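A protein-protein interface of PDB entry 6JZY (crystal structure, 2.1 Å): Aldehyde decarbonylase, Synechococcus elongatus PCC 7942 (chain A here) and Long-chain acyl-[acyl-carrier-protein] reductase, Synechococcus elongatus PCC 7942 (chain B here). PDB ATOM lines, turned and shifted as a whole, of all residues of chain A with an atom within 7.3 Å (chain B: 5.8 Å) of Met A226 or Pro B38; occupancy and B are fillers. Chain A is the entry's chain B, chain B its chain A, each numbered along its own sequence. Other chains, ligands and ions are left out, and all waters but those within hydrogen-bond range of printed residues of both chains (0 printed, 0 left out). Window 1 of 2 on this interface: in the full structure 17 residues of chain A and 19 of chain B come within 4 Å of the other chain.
OE1 of Glu A223 is in salt-bridge range of NZ of Lys B80, at 2.7 Å.
The side-chain amide nitrogen (ND2) of Asn B83 is in hydrogen-bond range of the side-chain carboxylate (OE2) of Glu A223.
O of Phe B33 is in hydrogen-bond range of OG of Ser B36 (3.5 Å).
NZ of Lys B80 sits at hydrogen-bond distance from O of Ala B37 (2.8 Å).
The backbone carbonyl oxygen (O) of Pro B38 sits at hydrogen-bond distance from the side-chain sulfur (SG) of Cys B63 (3.7 Å).
O of Gln B40 sits at hydrogen-bond distance from N of Glu B61, 2.9 Å away.
Ser B36 touches Val A222.
CA of Glu A223 touches O of Ser B36 (3.2 Å).
CE of Met A226 touches OH of Tyr B26 (3.8 Å).
Pro B38 touches Met A226.
CG1 of Ile A227 touches CB of Pro B38, at 3.6 Å.
Asn B83 touches Ile A227.
Met A244 touches Tyr B26 (O to CE1, 3.3 Å).
SD of Met A244 touches CG of Gln B40, at 3.6 Å.
Tyr B26 touches Ala A248.
Met A226 touches just these residues of chain B: Tyr B26 (3.8 Å) and Pro B38 (3.6 Å).
Printed residues of chain A within 4 Å of Asn B83: Glu A223 and Ile A227.
Printed residues of chain A within 4 Å of Tyr B26: Met A226 (3.8 Å), Met A244 (3.3 Å) and Ala A248 (3.9 Å).
Printed residues of chain B within 4 Å of Ala A248: Tyr B26.
The nearest residue of chain B that does not touch Met A226 is Ser B36 (4.1 Å).
The nearest printed residue of chain A that does not touch Asn B83 is Asp A224 (6.1 Å).
Of the 12 printed residues of chain B, 6 touch a printed residue of chain A.
Of the 25 printed residues of chain A, 6 touch a printed residue of chain B.
Hydrophobic or aromatic side chains of chain A that line the printed part of chain B: Val A222, Met A226, Ile A227, Met A244 and Ala A248.
Among the printed residues, Asp or Glu carboxylates within 4 Å of a Lys or Arg side-chain nitrogen of the other chain: Glu A223 with Lys B80 (2.7 Å).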
ATOM      1  N   CYS A 139      -2.470  12.274  26.083  1.00  0.00           N
ATOM      2  CA  CYS A 139      -3.704  12.974  26.431  1.00  0.00           C
ATOM      3  C   CYS A 139      -3.818  13.208  27.924  1.00  0.00           C
ATOM      4  O   CYS A 139      -4.300  14.262  28.351  1.00  0.00           O
ATOM      5  CB  CYS A 139      -4.886  12.191  25.909  1.00  0.00           C
ATOM      6  SG  CYS A 139      -4.866  12.227  24.143  1.00  0.00           S
ATOM      7  N   ALA A 143      -4.224  17.063  29.111  1.00  0.00           N
ATOM      8  CA  ALA A 143      -5.236  17.439  30.094  1.00  0.00           C
ATOM      9  C   ALA A 143      -4.600  18.011  31.353  1.00  0.00           C
ATOM     10  O   ALA A 143      -5.032  19.049  31.868  1.00  0.00           O
ATOM     11  CB  ALA A 143      -6.099  16.230  30.454  1.00  0.00           C
ATOM     12  N   LEU A 197      -7.840   2.369  29.264  1.00  0.00           N
ATOM     13  CA  LEU A 197      -8.552   3.595  29.609  1.00  0.00           C
ATOM     14  C   LEU A 197      -9.178   3.566  31.001  1.00  0.00           C
ATOM     15  O   LEU A 197      -9.147   4.615  31.666  1.00  0.00           O
ATOM     16  CB  LEU A 197      -9.605   3.904  28.535  1.00  0.00           C
ATOM     17  CG  LEU A 197     -10.309   5.247  28.721  1.00  0.00           C
ATOM     18  CD1 LEU A 197      -9.369   6.376  28.373  1.00  0.00           C
ATOM     19  CD2 LEU A 197     -11.535   5.303  27.856  1.00  0.00           C
ATOM     20  N   TRP A 201      -9.135   6.587  34.723  1.00  0.00           N
ATOM     21  CA  TRP A 201     -10.132   7.018  35.698  1.00  0.00           C
ATOM     22  C   TRP A 201      -9.677   6.706  37.118  1.00  0.00           C
ATOM     23  O   TRP A 201      -9.835   7.532  38.021  1.00  0.00           O
ATOM     24  CB  TRP A 201     -11.488   6.361  35.412  1.00  0.00           C
ATOM     25  CG  TRP A 201     -11.906   6.359  33.967  1.00  0.00           C
ATOM     26  CD1 TRP A 201     -12.437   5.307  33.271  1.00  0.00           C
ATOM     27  CD2 TRP A 201     -11.832   7.454  33.037  1.00  0.00           C
ATOM     28  NE1 TRP A 201     -12.697   5.680  31.970  1.00  0.00           N
ATOM     29  CE2 TRP A 201     -12.334   6.990  31.802  1.00  0.00           C
ATOM     30  CE3 TRP A 201     -11.385   8.775  33.127  1.00  0.00           C
ATOM     31  CZ2 TRP A 201     -12.404   7.804  30.673  1.00  0.00           C
ATOM     32  CZ3 TRP A 201     -11.443   9.575  32.002  1.00  0.00           C
ATOM     33  CH2 TRP A 201     -11.954   9.089  30.793  1.00  0.00           C
ATOM     34  N   SER A 220     -12.719  19.029  35.297  1.00  0.00           N
ATOM     35  CA  SER A 220     -12.023  19.605  34.148  1.00  0.00           C
ATOM     36  C   SER A 220     -10.970  18.664  33.584  1.00  0.00           C
ATOM     37  O   SER A 220     -10.720  18.671  32.372  1.00  0.00           O
ATOM     38  CB  SER A 220     -11.353  20.932  34.526  1.00  0.00           C
ATOM     39  OG  SER A 220     -12.193  22.041  34.256  1.00  0.00           O
ATOM     40  N   LEU A 221     -10.325  17.869  34.438  1.00  0.00           N
ATOM     41  CA  LEU A 221      -9.277  16.969  33.957  1.00  0.00           C
ATOM     42  C   LEU A 221      -9.858  15.880  33.063  1.00  0.00           C
ATOM     43  O   LEU A 221      -9.345  15.631  31.968  1.00  0.00           O
ATOM     44  CB  LEU A 221      -8.530  16.365  35.145  1.00  0.00           C
ATOM     45  CG  LEU A 221      -7.625  17.392  35.842  1.00  0.00           C
ATOM     46  CD1 LEU A 221      -7.264  16.946  37.247  1.00  0.00           C
ATOM     47  CD2 LEU A 221      -6.385  17.621  35.017  1.00  0.00           C
ATOM     48  N   VAL A 222     -10.941  15.233  33.518  1.00  0.00           N
ATOM     49  CA  VAL A 222     -11.678  14.262  32.700  1.00  0.00           C
ATOM     50  C   VAL A 222     -12.035  14.868  31.349  1.00  0.00           C
ATOM     51  O   VAL A 222     -11.799  14.274  30.292  1.00  0.00           O
ATOM     52  CB  VAL A 222     -12.953  13.793  33.435  1.00  0.00           C
ATOM     53  CG1 VAL A 222     -13.778  12.843  32.552  1.00  0.00           C
ATOM     54  CG2 VAL A 222     -12.625  13.124  34.773  1.00  0.00           C
ATOM     55  N   GLU A 223     -12.592  16.079  31.374  1.00  0.00           N
ATOM     56  CA  GLU A 223     -13.105  16.705  30.160  1.00  0.00           C
ATOM     57  C   GLU A 223     -11.994  16.968  29.157  1.00  0.00           C
ATOM     58  O   GLU A 223     -12.110  16.614  27.977  1.00  0.00           O
ATOM     59  CB  GLU A 223     -13.809  18.006  30.538  1.00  0.00           C
ATOM     60  CG  GLU A 223     -14.482  18.747  29.416  1.00  0.00           C
ATOM     61  CD  GLU A 223     -15.208  19.952  29.974  1.00  0.00           C
ATOM     62  OE1 GLU A 223     -16.339  19.771  30.470  1.00  0.00           O
ATOM     63  OE2 GLU A 223     -14.619  21.056  29.958  1.00  0.00           O
ATOM     64  N   ASP A 224     -10.910  17.610  29.603  1.00  0.00           N
ATOM     65  CA  ASP A 224      -9.774  17.849  28.720  1.00  0.00           C
ATOM     66  C   ASP A 224      -9.174  16.536  28.228  1.00  0.00           C
ATOM     67  O   ASP A 224      -8.812  16.412  27.051  1.00  0.00           O
ATOM     68  CB  ASP A 224      -8.732  18.699  29.449  1.00  0.00           C
ATOM     69  CG  ASP A 224      -9.026  20.191  29.338  1.00  0.00           C
ATOM     70  OD1 ASP A 224      -9.951  20.675  30.023  1.00  0.00           O
ATOM     71  OD2 ASP A 224      -8.376  20.871  28.520  1.00  0.00           O
ATOM     72  N   PHE A 225      -9.078  15.535  29.104  1.00  0.00           N
ATOM     73  CA  PHE A 225      -8.599  14.232  28.645  1.00  0.00           C
ATOM     74  C   PHE A 225      -9.506  13.680  27.551  1.00  0.00           C
ATOM     75  O   PHE A 225      -9.040  13.300  26.474  1.00  0.00           O
ATOM     76  CB  PHE A 225      -8.506  13.234  29.803  1.00  0.00           C
ATOM     77  CG  PHE A 225      -8.016  11.879  29.360  1.00  0.00           C
ATOM     78  CD1 PHE A 225      -6.649  11.606  29.307  1.00  0.00           C
ATOM     79  CD2 PHE A 225      -8.908  10.907  28.927  1.00  0.00           C
ATOM     80  CE1 PHE A 225      -6.182  10.376  28.866  1.00  0.00           C
ATOM     81  CE2 PHE A 225      -8.446   9.671  28.482  1.00  0.00           C
ATOM     82  CZ  PHE A 225      -7.077   9.407  28.456  1.00  0.00           C
ATOM     83  N   MET A 226     -10.816  13.654  27.803  1.00  0.00           N
ATOM     84  CA  MET A 226     -11.738  13.112  26.808  1.00  0.00           C
ATOM     85  C   MET A 226     -11.696  13.919  25.511  1.00  0.00           C
ATOM     86  O   MET A 226     -11.768  13.351  24.420  1.00  0.00           O
ATOM     87  CB  MET A 226     -13.154  13.071  27.391  1.00  0.00           C
ATOM     88  CG  MET A 226     -13.428  11.812  28.250  1.00  0.00           C
ATOM     89  SD  MET A 226     -15.106  11.768  28.978  1.00  0.00           S
ATOM     90  CE  MET A 226     -16.104  11.034  27.662  1.00  0.00           C
ATOM     91  N   ILE A 227     -11.550  15.245  25.600  1.00  0.00           N
ATOM     92  CA  ILE A 227     -11.431  16.053  24.383  1.00  0.00           C
ATOM     93  C   ILE A 227     -10.173  15.664  23.605  1.00  0.00           C
ATOM     94  O   ILE A 227     -10.216  15.395  22.397  1.00  0.00           O
ATOM     95  CB  ILE A 227     -11.427  17.554  24.730  1.00  0.00           C
ATOM     96  CG1 ILE A 227     -12.840  18.057  25.036  1.00  0.00           C
ATOM     97  CG2 ILE A 227     -10.882  18.356  23.554  1.00  0.00           C
ATOM     98  CD1 ILE A 227     -12.874  19.497  25.460  1.00  0.00           C
ATOM     99  N   ALA A 228      -9.022  15.643  24.284  1.00  0.00           N
ATOM    100  CA  ALA A 228      -7.778  15.276  23.603  1.00  0.00           C
ATOM    101  C   ALA A 228      -7.839  13.850  23.056  1.00  0.00           C
ATOM    102  O   ALA A 228      -7.467  13.601  21.901  1.00  0.00           O
ATOM    103  CB  ALA A 228      -6.595  15.435  24.556  1.00  0.00           C
ATOM    104  N   TYR A 229      -8.313  12.902  23.870  1.00  0.00           N
ATOM    105  CA  TYR A 229      -8.360  11.503  23.443  1.00  0.00           C
ATOM    106  C   TYR A 229      -9.357  11.314  22.315  1.00  0.00           C
ATOM    107  O   TYR A 229      -9.092  10.570  21.368  1.00  0.00           O
ATOM    108  CB  TYR A 229      -8.718  10.611  24.632  1.00  0.00           C
ATOM    109  CG  TYR A 229      -8.503   9.106  24.463  1.00  0.00           C
ATOM    110  CD1 TYR A 229      -7.235   8.578  24.293  1.00  0.00           C
ATOM    111  CD2 TYR A 229      -9.571   8.217  24.561  1.00  0.00           C
ATOM    112  CE1 TYR A 229      -7.022   7.210  24.176  1.00  0.00           C
ATOM    113  CE2 TYR A 229      -9.369   6.843  24.457  1.00  0.00           C
ATOM    114  CZ  TYR A 229      -8.093   6.342  24.258  1.00  0.00           C
ATOM    115  OH  TYR A 229      -7.893   4.975  24.151  1.00  0.00           O
ATOM    116  N   GLY A 230     -10.508  11.987  22.391  1.00  0.00           N
ATOM    117  CA  GLY A 230     -11.499  11.837  21.341  1.00  0.00           C
ATOM    118  C   GLY A 230     -10.981  12.305  19.996  1.00  0.00           C
ATOM    119  O   GLY A 230     -11.167  11.640  18.974  1.00  0.00           O
ATOM    120  N   GLU A 231     -10.312  13.456  19.987  1.00  0.00           N
ATOM    121  CA  GLU A 231      -9.817  14.000  18.728  1.00  0.00           C
ATOM    122  C   GLU A 231      -8.766  13.089  18.098  1.00  0.00           C
ATOM    123  O   GLU A 231      -8.699  12.948  16.872  1.00  0.00           O
ATOM    124  CB  GLU A 231      -9.251  15.396  18.961  1.00  0.00           C
ATOM    125  CG  GLU A 231      -8.134  15.760  18.005  1.00  0.00           C
ATOM    126  CD  GLU A 231      -7.841  17.247  17.988  1.00  0.00           C
ATOM    127  OE1 GLU A 231      -6.821  17.636  17.376  1.00  0.00           O
ATOM    128  OE2 GLU A 231      -8.621  18.021  18.588  1.00  0.00           O
ATOM    129  N   ALA A 232      -7.933  12.445  18.912  1.00  0.00           N
ATOM    130  CA  ALA A 232      -6.954  11.530  18.332  1.00  0.00           C
ATOM    131  C   ALA A 232      -7.654  10.323  17.728  1.00  0.00           C
ATOM    132  O   ALA A 232      -7.354   9.927  16.600  1.00  0.00           O
ATOM    133  CB  ALA A 232      -5.912  11.113  19.374  1.00  0.00           C
ATOM    134  N   LEU A 233      -8.624   9.748  18.446  1.00  0.00           N
ATOM    135  CA  LEU A 233      -9.337   8.600  17.902  1.00  0.00           C
ATOM    136  C   LEU A 233     -10.050   8.960  16.614  1.00  0.00           C
ATOM    137  O   LEU A 233     -10.160   8.126  15.706  1.00  0.00           O
ATOM    138  CB  LEU A 233     -10.338   8.053  18.916  1.00  0.00           C
ATOM    139  CG  LEU A 233      -9.778   7.631  20.269  1.00  0.00           C
ATOM    140  CD1 LEU A 233     -10.897   7.125  21.135  1.00  0.00           C
ATOM    141  CD2 LEU A 233      -8.724   6.537  20.058  1.00  0.00           C
ATOM    142  N   ILE A 243     -16.108   6.391  18.870  1.00  0.00           N
ATOM    143  CA  ILE A 243     -15.409   7.235  19.839  1.00  0.00           C
ATOM    144  C   ILE A 243     -16.209   7.351  21.130  1.00  0.00           C
ATOM    145  O   ILE A 243     -15.668   7.212  22.233  1.00  0.00           O
ATOM    146  CB  ILE A 243     -15.128   8.626  19.244  1.00  0.00           C
ATOM    147  CG1 ILE A 243     -14.043   8.553  18.170  1.00  0.00           C
ATOM    148  CG2 ILE A 243     -14.723   9.589  20.350  1.00  0.00           C
ATOM    149  CD1 ILE A 243     -13.977   9.815  17.329  1.00  0.00           C
ATOM    150  N   MET A 244     -17.505   7.634  21.022  1.00  0.00           N
ATOM    151  CA  MET A 244     -18.279   7.813  22.242  1.00  0.00           C
ATOM    152  C   MET A 244     -18.392   6.512  23.030  1.00  0.00           C
ATOM    153  O   MET A 244     -18.427   6.541  24.265  1.00  0.00           O
ATOM    154  CB  MET A 244     -19.647   8.398  21.911  1.00  0.00           C
ATOM    155  CG  MET A 244     -19.549   9.887  21.575  1.00  0.00           C
ATOM    156  SD  MET A 244     -21.069  10.663  20.993  1.00  0.00           S
ATOM    157  CE  MET A 244     -22.264   9.513  21.635  1.00  0.00           C
ATOM    158  N   MET A 246     -15.900   4.121  22.968  1.00  0.00           N
ATOM    159  CA  MET A 246     -14.564   3.861  23.494  1.00  0.00           C
ATOM    160  C   MET A 246     -14.188   4.844  24.593  1.00  0.00           C
ATOM    161  O   MET A 246     -13.585   4.453  25.598  1.00  0.00           O
ATOM    162  CB  MET A 246     -13.539   3.910  22.360  1.00  0.00           C
ATOM    163  CG  MET A 246     -13.732   2.835  21.309  1.00  0.00           C
ATOM    164  SD  MET A 246     -12.726   3.218  19.881  1.00  0.00           S
ATOM    165  CE  MET A 246     -11.113   3.019  20.616  1.00  0.00           C
ATOM    166  N   SER A 247     -14.534   6.124  24.420  1.00  0.00           N
ATOM    167  CA  SER A 247     -14.058   7.168  25.324  1.00  0.00           C
ATOM    168  C   SER A 247     -14.678   7.076  26.708  1.00  0.00           C
ATOM    169  O   SER A 247     -14.100   7.592  27.671  1.00  0.00           O
ATOM    170  CB  SER A 247     -14.353   8.550  24.743  1.00  0.00           C
ATOM    171  OG  SER A 247     -14.209   8.533  23.338  1.00  0.00           O
ATOM    172  N   ALA A 248     -15.837   6.446  26.835  1.00  0.00           N
ATOM    173  CA  ALA A 248     -16.506   6.372  28.120  1.00  0.00           C
ATOM    174  C   ALA A 248     -16.327   5.017  28.781  1.00  0.00           C
ATOM    175  O   ALA A 248     -16.936   4.759  29.823  1.00  0.00           O
ATOM    176  CB  ALA A 248     -17.990   6.704  27.954  1.00  0.00           C
ATOM    177  N   TYR A 249     -15.490   4.153  28.213  1.00  0.00           N
ATOM    178  CA  TYR A 249     -15.331   2.817  28.764  1.00  0.00           C
ATOM    179  C   TYR A 249     -14.687   2.893  30.146  1.00  0.00           C
ATOM    180  O   TYR A 249     -13.698   3.599  30.343  1.00  0.00           O
ATOM    181  CB  TYR A 249     -14.496   1.948  27.825  1.00  0.00           C
ATOM    182  CG  TYR A 249     -14.498   0.504  28.228  1.00  0.00           C
ATOM    183  CD1 TYR A 249     -15.460  -0.367  27.740  1.00  0.00           C
ATOM    184  CD2 TYR A 249     -13.547   0.010  29.114  1.00  0.00           C
ATOM    185  CE1 TYR A 249     -15.475  -1.702  28.123  1.00  0.00           C
ATOM    186  CE2 TYR A 249     -13.547  -1.325  29.500  1.00  0.00           C
ATOM    187  CZ  TYR A 249     -14.515  -2.176  29.003  1.00  0.00           C
ATOM    188  OH  TYR A 249     -14.508  -3.504  29.386  1.00  0.00           O
ATOM    189  N   LEU A 251     -15.880   4.396  32.683  1.00  0.00           N
ATOM    190  CA  LEU A 251     -16.334   5.590  33.389  1.00  0.00           C
ATOM    191  C   LEU A 251     -17.726   5.368  33.980  1.00  0.00           C
ATOM    192  O   LEU A 251     -17.867   4.971  35.140  1.00  0.00           O
ATOM    193  CB  LEU A 251     -16.338   6.806  32.443  1.00  0.00           C
ATOM    194  CG  LEU A 251     -16.206   8.199  33.079  1.00  0.00           C
ATOM    195  CD1 LEU A 251     -14.968   8.262  33.955  1.00  0.00           C
ATOM    196  CD2 LEU A 251     -16.182   9.330  32.041  1.00  0.00           C
ATOM    197  N   TYR B  26     -23.661   6.569  27.759  1.00  0.00           N
ATOM    198  CA  TYR B  26     -24.032   7.974  27.910  1.00  0.00           C
ATOM    199  C   TYR B  26     -25.430   8.173  28.500  1.00  0.00           C
ATOM    200  O   TYR B  26     -25.783   9.313  28.808  1.00  0.00           O
ATOM    201  CB  TYR B  26     -23.948   8.669  26.548  1.00  0.00           C
ATOM    202  CG  TYR B  26     -22.591   9.231  26.159  1.00  0.00           C
ATOM    203  CD1 TYR B  26     -21.482   8.404  26.009  1.00  0.00           C
ATOM    204  CD2 TYR B  26     -22.427  10.596  25.925  1.00  0.00           C
ATOM    205  CE1 TYR B  26     -20.236   8.921  25.652  1.00  0.00           C
ATOM    206  CE2 TYR B  26     -21.198  11.121  25.572  1.00  0.00           C
ATOM    207  CZ  TYR B  26     -20.100  10.282  25.434  1.00  0.00           C
ATOM    208  OH  TYR B  26     -18.868  10.807  25.080  1.00  0.00           O
ATOM    209  N   PHE B  33     -21.388  13.249  34.854  1.00  0.00           N
ATOM    210  CA  PHE B  33     -20.834  12.760  33.596  1.00  0.00           C
ATOM    211  C   PHE B  33     -20.986  13.790  32.483  1.00  0.00           C
ATOM    212  O   PHE B  33     -20.044  14.036  31.720  1.00  0.00           O
ATOM    213  CB  PHE B  33     -21.506  11.463  33.179  1.00  0.00           C
ATOM    214  CG  PHE B  33     -21.201  11.078  31.770  1.00  0.00           C
ATOM    215  CD1 PHE B  33     -19.956  10.580  31.440  1.00  0.00           C
ATOM    216  CD2 PHE B  33     -22.145  11.234  30.765  1.00  0.00           C
ATOM    217  CE1 PHE B  33     -19.658  10.229  30.146  1.00  0.00           C
ATOM    218  CE2 PHE B  33     -21.852  10.886  29.465  1.00  0.00           C
ATOM    219  CZ  PHE B  33     -20.605  10.380  29.154  1.00  0.00           C
ATOM    220  N   SER B  36     -18.491  16.698  32.530  1.00  0.00           N
ATOM    221  CA  SER B  36     -17.159  16.517  31.965  1.00  0.00           C
ATOM    222  C   SER B  36     -17.188  15.936  30.552  1.00  0.00           C
ATOM    223  O   SER B  36     -16.133  15.586  30.011  1.00  0.00           O
ATOM    224  CB  SER B  36     -16.296  15.659  32.898  1.00  0.00           C
ATOM    225  OG  SER B  36     -16.906  14.412  33.151  1.00  0.00           O
ATOM    226  N   ALA B  37     -18.357  15.859  29.923  1.00  0.00           N
ATOM    227  CA  ALA B  37     -18.423  15.259  28.599  1.00  0.00           C
ATOM    228  C   ALA B  37     -17.930  16.231  27.525  1.00  0.00           C
ATOM    229  O   ALA B  37     -18.151  17.441  27.620  1.00  0.00           O
ATOM    230  CB  ALA B  37     -19.853  14.816  28.284  1.00  0.00           C
ATOM    231  N   PRO B  38     -17.264  15.721  26.494  1.00  0.00           N
ATOM    232  CA  PRO B  38     -16.771  16.578  25.416  1.00  0.00           C
ATOM    233  C   PRO B  38     -17.855  16.839  24.384  1.00  0.00           C
ATOM    234  O   PRO B  38     -18.797  16.044  24.241  1.00  0.00           O
ATOM    235  CB  PRO B  38     -15.628  15.745  24.813  1.00  0.00           C
ATOM    236  CG  PRO B  38     -16.114  14.343  24.975  1.00  0.00           C
ATOM    237  CD  PRO B  38     -16.823  14.321  26.321  1.00  0.00           C
ATOM    238  N   PRO B  39     -17.742  17.924  23.622  1.00  0.00           N
ATOM    239  CA  PRO B  39     -18.674  18.147  22.510  1.00  0.00           C
ATOM    240  C   PRO B  39     -18.521  17.073  21.446  1.00  0.00           C
ATOM    241  O   PRO B  39     -17.443  16.512  21.255  1.00  0.00           O
ATOM    242  CB  PRO B  39     -18.241  19.508  21.963  1.00  0.00           C
ATOM    243  CG  PRO B  39     -16.753  19.538  22.239  1.00  0.00           C
ATOM    244  CD  PRO B  39     -16.607  18.869  23.591  1.00  0.00           C
ATOM    245  N   GLN B  40     -19.600  16.811  20.713  1.00  0.00           N
ATOM    246  CA  GLN B  40     -19.535  15.790  19.673  1.00  0.00           C
ATOM    247  C   GLN B  40     -20.360  16.222  18.473  1.00  0.00           C
ATOM    248  O   GLN B  40     -21.466  16.738  18.643  1.00  0.00           O
ATOM    249  CB  GLN B  40     -20.060  14.436  20.177  1.00  0.00           C
ATOM    250  CG  GLN B  40     -19.192  13.735  21.206  1.00  0.00           C
ATOM    251  CD  GLN B  40     -17.826  13.338  20.677  1.00  0.00           C
ATOM    252  OE1 GLN B  40     -17.489  13.561  19.509  1.00  0.00           O
ATOM    253  NE2 GLN B  40     -17.018  12.748  21.552  1.00  0.00           N
ATOM    254  N   GLU B  61     -23.483  18.479  19.719  1.00  0.00           N
ATOM    255  CA  GLU B  61     -24.045  18.387  21.065  1.00  0.00           C
ATOM    256  C   GLU B  61     -23.043  19.011  22.032  1.00  0.00           C
ATOM    257  O   GLU B  61     -21.914  18.526  22.167  1.00  0.00           O
ATOM    258  CB  GLU B  61     -24.350  16.934  21.417  1.00  0.00           C
ATOM    259  CG  GLU B  61     -24.898  16.742  22.823  1.00  0.00           C
ATOM    260  CD  GLU B  61     -26.029  17.713  23.136  1.00  0.00           C
ATOM    261  OE1 GLU B  61     -26.981  17.818  22.333  1.00  0.00           O
ATOM    262  OE2 GLU B  61     -25.957  18.386  24.182  1.00  0.00           O
ATOM    263  N   SER B  62     -23.422  20.130  22.636  1.00  0.00           N
ATOM    264  CA  SER B  62     -22.590  20.820  23.607  1.00  0.00           C
ATOM    265  C   SER B  62     -22.562  20.138  24.968  1.00  0.00           C
ATOM    266  O   SER B  62     -21.632  20.381  25.742  1.00  0.00           O
ATOM    267  CB  SER B  62     -23.104  22.244  23.816  1.00  0.00           C
ATOM    268  OG  SER B  62     -24.375  22.214  24.460  1.00  0.00           O
ATOM    269  N   CYS B  63     -23.575  19.333  25.290  1.00  0.00           N
ATOM    270  CA  CYS B  63     -23.720  18.654  26.576  1.00  0.00           C
ATOM    271  C   CYS B  63     -24.040  19.607  27.716  1.00  0.00           C
ATOM    272  O   CYS B  63     -23.926  19.233  28.885  1.00  0.00           O
ATOM    273  CB  CYS B  63     -22.474  17.829  26.931  1.00  0.00           C
ATOM    274  SG  CYS B  63     -22.177  16.449  25.786  1.00  0.00           S
ATOM    275  N   LYS B  80     -18.901  24.103  28.592  1.00  0.00           N
ATOM    276  CA  LYS B  80     -19.689  23.416  27.570  1.00  0.00           C
ATOM    277  C   LYS B  80     -19.770  24.264  26.309  1.00  0.00           C
ATOM    278  O   LYS B  80     -19.590  23.766  25.195  1.00  0.00           O
ATOM    279  CB  LYS B  80     -21.099  23.087  28.091  1.00  0.00           C
ATOM    280  CG  LYS B  80     -21.194  22.149  29.300  1.00  0.00           C
ATOM    281  CD  LYS B  80     -20.622  20.766  29.010  1.00  0.00           C
ATOM    282  CE  LYS B  80     -19.258  20.553  29.679  1.00  0.00           C
ATOM    283  NZ  LYS B  80     -18.861  19.078  29.736  1.00  0.00           N
ATOM    284  N   ASN B  83     -16.109  24.856  24.701  1.00  0.00           N
ATOM    285  CA  ASN B  83     -15.642  23.614  24.085  1.00  0.00           C
ATOM    286  C   ASN B  83     -16.395  23.337  22.793  1.00  0.00           C
ATOM    287  O   ASN B  83     -15.799  22.927  21.791  1.00  0.00           O
ATOM    288  CB  ASN B  83     -15.811  22.434  25.037  1.00  0.00           C
ATOM    289  CG  ASN B  83     -14.970  22.556  26.296  1.00  0.00           C
ATOM    290  OD1 ASN B  83     -13.999  23.323  26.352  1.00  0.00           O
ATOM    291  ND2 ASN B  83     -15.344  21.794  27.324  1.00  0.00           N
